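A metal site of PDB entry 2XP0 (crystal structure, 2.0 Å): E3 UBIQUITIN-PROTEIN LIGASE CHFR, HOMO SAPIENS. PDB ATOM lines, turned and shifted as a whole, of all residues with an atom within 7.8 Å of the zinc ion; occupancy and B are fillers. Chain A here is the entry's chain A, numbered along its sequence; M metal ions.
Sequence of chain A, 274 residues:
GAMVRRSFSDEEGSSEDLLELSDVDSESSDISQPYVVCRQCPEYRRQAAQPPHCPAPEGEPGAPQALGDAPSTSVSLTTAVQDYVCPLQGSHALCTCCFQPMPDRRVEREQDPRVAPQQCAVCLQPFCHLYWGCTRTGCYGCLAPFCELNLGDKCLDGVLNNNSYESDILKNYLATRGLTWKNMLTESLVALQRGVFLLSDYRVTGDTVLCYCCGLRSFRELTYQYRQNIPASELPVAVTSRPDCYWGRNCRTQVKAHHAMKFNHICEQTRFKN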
ATOM      1  N   ASN A 163      -2.972 -24.433 -15.761  1.00  0.00           N
ATOM      2  CA  ASN A 163      -3.547 -24.334 -17.102  1.00  0.00           C
ATOM      3  C   ASN A 163      -5.040 -24.063 -16.923  1.00  0.00           C
ATOM      4  O   ASN A 163      -5.784 -24.940 -16.472  1.00  0.00           O
ATOM      5  CB  ASN A 163      -3.303 -25.665 -17.831  1.00  0.00           C
ATOM      6  CG  ASN A 163      -3.919 -25.726 -19.227  1.00  0.00           C
ATOM      7  OD1 ASN A 163      -4.997 -25.190 -19.484  1.00  0.00           O
ATOM      8  ND2 ASN A 163      -3.245 -26.442 -20.118  1.00  0.00           N
ATOM      9  N   ASP A 244      -3.328 -35.497 -27.759  1.00  0.00           N
ATOM     10  CA  ASP A 244      -2.381 -35.305 -26.680  1.00  0.00           C
ATOM     11  C   ASP A 244      -1.244 -34.432 -27.168  1.00  0.00           C
ATOM     12  O   ASP A 244      -0.731 -34.629 -28.275  1.00  0.00           O
ATOM     13  CB  ASP A 244      -1.786 -36.642 -26.234  1.00  0.00           C
ATOM     14  CG  ASP A 244      -2.755 -37.505 -25.458  1.00  0.00           C
ATOM     15  OD1 ASP A 244      -3.916 -37.084 -25.245  1.00  0.00           O
ATOM     16  OD2 ASP A 244      -2.340 -38.606 -25.061  1.00  0.00           O
ATOM     17  N   CYS A 245      -0.811 -33.490 -26.339  1.00  0.00           N
ATOM     18  CA  CYS A 245       0.422 -32.760 -26.617  1.00  0.00           C
ATOM     19  C   CYS A 245       1.619 -33.696 -26.423  1.00  0.00           C
ATOM     20  O   CYS A 245       1.722 -34.376 -25.398  1.00  0.00           O
ATOM     21  CB  CYS A 245       0.582 -31.532 -25.709  1.00  0.00           C
ATOM     22  SG  CYS A 245       2.142 -30.629 -26.049  1.00  0.00           S
ATOM     23  N   TYR A 246       2.510 -33.699 -27.406  1.00  0.00           N
ATOM     24  CA  TYR A 246       3.747 -34.486 -27.359  1.00  0.00           C
ATOM     25  C   TYR A 246       4.512 -34.318 -26.037  1.00  0.00           C
ATOM     26  O   TYR A 246       5.102 -35.270 -25.522  1.00  0.00           O
ATOM     27  CB  TYR A 246       4.642 -34.077 -28.535  1.00  0.00           C
ATOM     28  CG  TYR A 246       5.893 -34.904 -28.715  1.00  0.00           C
ATOM     29  CD1 TYR A 246       7.069 -34.554 -28.078  1.00  0.00           C
ATOM     30  CD2 TYR A 246       5.905 -36.022 -29.538  1.00  0.00           C
ATOM     31  CE1 TYR A 246       8.221 -35.300 -28.234  1.00  0.00           C
ATOM     32  CE2 TYR A 246       7.046 -36.776 -29.715  1.00  0.00           C
ATOM     33  CZ  TYR A 246       8.200 -36.400 -29.058  1.00  0.00           C
ATOM     34  OH  TYR A 246       9.353 -37.146 -29.214  1.00  0.00           O
ATOM     35  N   TRP A 247       4.496 -33.104 -25.497  1.00  0.00           N
ATOM     36  CA  TRP A 247       5.279 -32.748 -24.317  1.00  0.00           C
ATOM     37  C   TRP A 247       4.572 -33.042 -22.987  1.00  0.00           C
ATOM     38  O   TRP A 247       5.208 -33.004 -21.932  1.00  0.00           O
ATOM     39  CB  TRP A 247       5.688 -31.255 -24.357  1.00  0.00           C
ATOM     40  CG  TRP A 247       6.336 -30.904 -25.669  1.00  0.00           C
ATOM     41  CD1 TRP A 247       5.781 -30.172 -26.686  1.00  0.00           C
ATOM     42  CD2 TRP A 247       7.626 -31.314 -26.127  1.00  0.00           C
ATOM     43  NE1 TRP A 247       6.668 -30.081 -27.735  1.00  0.00           N
ATOM     44  CE2 TRP A 247       7.810 -30.774 -27.422  1.00  0.00           C
ATOM     45  CE3 TRP A 247       8.657 -32.079 -25.568  1.00  0.00           C
ATOM     46  CZ2 TRP A 247       8.965 -30.970 -28.163  1.00  0.00           C
ATOM     47  CZ3 TRP A 247       9.826 -32.278 -26.311  1.00  0.00           C
ATOM     48  CH2 TRP A 247       9.957 -31.724 -27.584  1.00  0.00           C
ATOM     49  N   GLY A 248       3.266 -33.308 -23.031  1.00  0.00           N
ATOM     50  CA  GLY A 248       2.559 -33.797 -21.861  1.00  0.00           C
ATOM     51  C   GLY A 248       2.330 -32.733 -20.794  1.00  0.00           C
ATOM     52  O   GLY A 248       2.357 -31.548 -21.090  1.00  0.00           O
ATOM     53  N   ARG A 249       2.135 -33.179 -19.552  1.00  0.00           N
ATOM     54  CA  ARG A 249       1.699 -32.331 -18.452  1.00  0.00           C
ATOM     55  C   ARG A 249       2.660 -31.180 -18.139  1.00  0.00           C
ATOM     56  O   ARG A 249       2.244 -30.139 -17.617  1.00  0.00           O
ATOM     57  CB  ARG A 249       1.473 -33.173 -17.186  1.00  0.00           C
ATOM     58  CG  ARG A 249       2.691 -34.008 -16.805  1.00  0.00           C
ATOM     59  CD  ARG A 249       2.356 -35.097 -15.772  1.00  0.00           C
ATOM     60  NE  ARG A 249       1.901 -34.534 -14.505  1.00  0.00           N
ATOM     61  CZ  ARG A 249       1.613 -35.252 -13.425  1.00  0.00           C
ATOM     62  NH1 ARG A 249       1.748 -36.569 -13.449  1.00  0.00           N
ATOM     63  NH2 ARG A 249       1.207 -34.653 -12.307  1.00  0.00           N
ATOM     64  N   ASN A 250       3.934 -31.371 -18.483  1.00  0.00           N
ATOM     65  CA  ASN A 250       4.946 -30.362 -18.206  1.00  0.00           C
ATOM     66  C   ASN A 250       5.215 -29.389 -19.337  1.00  0.00           C
ATOM     67  O   ASN A 250       6.054 -28.497 -19.216  1.00  0.00           O
ATOM     68  CB  ASN A 250       6.239 -31.001 -17.700  1.00  0.00           C
ATOM     69  CG  ASN A 250       6.014 -31.740 -16.389  1.00  0.00           C
ATOM     70  OD1 ASN A 250       5.350 -31.214 -15.497  1.00  0.00           O
ATOM     71  ND2 ASN A 250       6.522 -32.968 -16.297  1.00  0.00           N
ATOM     72  N   CYS A 251       4.464 -29.528 -20.428  1.00  0.00           N
ATOM     73  CA  CYS A 251       4.576 -28.627 -21.561  1.00  0.00           C
ATOM     74  C   CYS A 251       4.655 -27.147 -21.122  1.00  0.00           C
ATOM     75  O   CYS A 251       3.817 -26.682 -20.341  1.00  0.00           O
ATOM     76  CB  CYS A 251       3.389 -28.819 -22.509  1.00  0.00           C
ATOM     77  SG  CYS A 251       3.445 -27.684 -23.905  1.00  0.00           S
ATOM     78  N   ARG A 252       5.633 -26.421 -21.634  1.00  0.00           N
ATOM     79  CA  ARG A 252       5.777 -25.005 -21.297  1.00  0.00           C
ATOM     80  C   ARG A 252       4.845 -24.105 -22.116  1.00  0.00           C
ATOM     81  O   ARG A 252       4.656 -22.947 -21.772  1.00  0.00           O
ATOM     82  CB  ARG A 252       7.227 -24.555 -21.509  1.00  0.00           C
ATOM     83  CG  ARG A 252       8.281 -25.454 -20.852  1.00  0.00           C
ATOM     84  CD  ARG A 252       8.140 -25.445 -19.352  1.00  0.00           C
ATOM     85  NE  ARG A 252       9.289 -24.802 -18.709  1.00  0.00           N
ATOM     86  CZ  ARG A 252      10.098 -25.407 -17.835  1.00  0.00           C
ATOM     87  NH1 ARG A 252      11.124 -24.739 -17.320  1.00  0.00           N
ATOM     88  NH2 ARG A 252       9.890 -26.668 -17.480  1.00  0.00           N
ATOM     89  N   THR A 253       4.266 -24.635 -23.184  1.00  0.00           N
ATOM     90  CA  THR A 253       3.460 -23.829 -24.099  1.00  0.00           C
ATOM     91  C   THR A 253       2.017 -23.708 -23.652  1.00  0.00           C
ATOM     92  O   THR A 253       1.256 -22.899 -24.189  1.00  0.00           O
ATOM     93  CB  THR A 253       3.464 -24.412 -25.519  1.00  0.00           C
ATOM     94  OG1 THR A 253       4.787 -24.777 -25.861  1.00  0.00           O
ATOM     95  CG2 THR A 253       2.907 -23.396 -26.550  1.00  0.00           C
ATOM     96  N   GLN A 254       1.620 -24.534 -22.692  1.00  0.00           N
ATOM     97  CA  GLN A 254       0.231 -24.572 -22.295  1.00  0.00           C
ATOM     98  C   GLN A 254      -0.187 -23.318 -21.521  1.00  0.00           C
ATOM     99  O   GLN A 254      -1.362 -23.134 -21.256  1.00  0.00           O
ATOM    100  CB  GLN A 254      -0.109 -25.866 -21.533  1.00  0.00           C
ATOM    101  CG  GLN A 254       0.516 -25.981 -20.177  1.00  0.00           C
ATOM    102  CD  GLN A 254       0.343 -27.376 -19.593  1.00  0.00           C
ATOM    103  OE1 GLN A 254      -0.783 -27.861 -19.395  1.00  0.00           O
ATOM    104  NE2 GLN A 254       1.461 -28.006 -19.269  1.00  0.00           N
ATOM    105  N   VAL A 255       0.749 -22.427 -21.215  1.00  0.00           N
ATOM    106  CA  VAL A 255       0.328 -21.153 -20.645  1.00  0.00           C
ATOM    107  C   VAL A 255      -0.274 -20.249 -21.717  1.00  0.00           C
ATOM    108  O   VAL A 255      -0.848 -19.213 -21.400  1.00  0.00           O
ATOM    109  CB  VAL A 255       1.451 -20.424 -19.907  1.00  0.00           C
ATOM    110  CG1 VAL A 255       2.113 -21.363 -18.900  1.00  0.00           C
ATOM    111  CG2 VAL A 255       2.468 -19.873 -20.896  1.00  0.00           C
ATOM    112  N   HIS A 259      -2.748 -22.837 -27.553  1.00  0.00           N
ATOM    113  CA  HIS A 259      -2.140 -24.145 -27.406  1.00  0.00           C
ATOM    114  C   HIS A 259      -2.898 -25.004 -26.385  1.00  0.00           C
ATOM    115  O   HIS A 259      -3.121 -26.189 -26.614  1.00  0.00           O
ATOM    116  CB  HIS A 259      -0.665 -24.017 -27.001  1.00  0.00           C
ATOM    117  CG  HIS A 259       0.066 -25.326 -26.991  1.00  0.00           C
ATOM    118  ND1 HIS A 259       0.542 -25.919 -28.139  1.00  0.00           N
ATOM    119  CD2 HIS A 259       0.389 -26.152 -25.971  1.00  0.00           C
ATOM    120  CE1 HIS A 259       1.129 -27.070 -27.825  1.00  0.00           C
ATOM    121  NE2 HIS A 259       1.049 -27.224 -26.520  1.00  0.00           N
ATOM    122  N   ALA A 260      -3.273 -24.399 -25.260  1.00  0.00           N
ATOM    123  CA  ALA A 260      -4.017 -25.080 -24.197  1.00  0.00           C
ATOM    124  C   ALA A 260      -5.352 -25.628 -24.693  1.00  0.00           C
ATOM    125  O   ALA A 260      -5.762 -26.730 -24.333  1.00  0.00           O
ATOM    126  CB  ALA A 260      -4.251 -24.138 -23.037  1.00  0.00           C
ATOM    127  N   PHE A 263      -4.690 -28.777 -27.548  1.00  0.00           N
ATOM    128  CA  PHE A 263      -4.141 -30.088 -27.187  1.00  0.00           C
ATOM    129  C   PHE A 263      -4.526 -30.482 -25.768  1.00  0.00           C
ATOM    130  O   PHE A 263      -4.596 -29.640 -24.889  1.00  0.00           O
ATOM    131  CB  PHE A 263      -2.618 -30.056 -27.233  1.00  0.00           C
ATOM    132  CG  PHE A 263      -2.054 -29.774 -28.605  1.00  0.00           C
ATOM    133  CD1 PHE A 263      -1.684 -28.488 -28.972  1.00  0.00           C
ATOM    134  CD2 PHE A 263      -1.885 -30.809 -29.521  1.00  0.00           C
ATOM    135  CE1 PHE A 263      -1.165 -28.241 -30.232  1.00  0.00           C
ATOM    136  CE2 PHE A 263      -1.366 -30.567 -30.774  1.00  0.00           C
ATOM    137  CZ  PHE A 263      -1.002 -29.275 -31.135  1.00  0.00           C
ATOM    138  N   ASN A 264      -4.712 -31.786 -25.550  1.00  0.00           N
ATOM    139  CA  ASN A 264      -4.887 -32.309 -24.189  1.00  0.00           C
ATOM    140  C   ASN A 264      -3.537 -32.331 -23.473  1.00  0.00           C
ATOM    141  O   ASN A 264      -2.545 -32.821 -24.036  1.00  0.00           O
ATOM    142  CB  ASN A 264      -5.477 -33.715 -24.242  1.00  0.00           C
ATOM    143  CG  ASN A 264      -5.406 -34.428 -22.896  1.00  0.00           C
ATOM    144  OD1 ASN A 264      -5.763 -33.873 -21.863  1.00  0.00           O
ATOM    145  ND2 ASN A 264      -4.942 -35.681 -22.917  1.00  0.00           N
ATOM    146  N   HIS A 265      -3.480 -31.780 -22.258  1.00  0.00           N
ATOM    147  CA  HIS A 265      -2.255 -31.814 -21.467  1.00  0.00           C
ATOM    148  C   HIS A 265      -2.384 -32.707 -20.226  1.00  0.00           C
ATOM    149  O   HIS A 265      -1.516 -32.694 -19.335  1.00  0.00           O
ATOM    150  CB  HIS A 265      -1.759 -30.409 -21.123  1.00  0.00           C
ATOM    151  CG  HIS A 265      -1.172 -29.691 -22.306  1.00  0.00           C
ATOM    152  ND1 HIS A 265      -1.939 -28.936 -23.171  1.00  0.00           N
ATOM    153  CD2 HIS A 265       0.092 -29.625 -22.776  1.00  0.00           C
ATOM    154  CE1 HIS A 265      -1.174 -28.442 -24.128  1.00  0.00           C
ATOM    155  NE2 HIS A 265       0.063 -28.834 -23.901  1.00  0.00           N
ATOM    156  N   CYS A 267      -1.653 -35.871 -19.832  1.00  0.00           N
ATOM    157  CA  CYS A 267      -0.946 -36.997 -20.398  1.00  0.00           C
ATOM    158  C   CYS A 267       0.524 -36.835 -20.043  1.00  0.00           C
ATOM    159  O   CYS A 267       0.923 -35.796 -19.511  1.00  0.00           O
ATOM    160  CB  CYS A 267      -1.153 -37.082 -21.925  1.00  0.00           C
ATOM    161  SG  CYS A 267      -0.712 -35.594 -22.885  1.00  0.00           S
HETATM  162 ZN    ZN M   1       1.668 -28.600 -25.097  1.00  0.00          ZN
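The backbone NH (N) of Cys 245 is in hydrogen-bond range of the backbone carbonyl oxygen (O) of Asn 264.
SG of Cys 267 sits at hydrogen-bond distance from O of Cys 245 (3.7 Å).
A ring nitrogen (ND1) of His 265 lies within hydrogen-bond range of the backbone carbonyl oxygen of Phe 263 (3.2 Å).
SG of Cys 245 lies close to N of Trp 247 (3.5 Å).
SG of Cys 251 sits close to N of Thr 253, at 3.2 Å.
The backbone carbonyl oxygen of Cys 251 sits at hydrogen-bond distance from the side-chain amide nitrogen of Gln 254 (2.9 Å).
Of the 19 residues printed, 4 come within 4 Å of the zinc ion.
The zinc ion is bound by NE2 of His 265 (2.0 Å), NE2 of His 259 (2.1 Å), SG of Cys 245 (2.3 Å) and SG of Cys 251 (2.3 Å).
The zinc ion has four donor atoms within binding distance.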
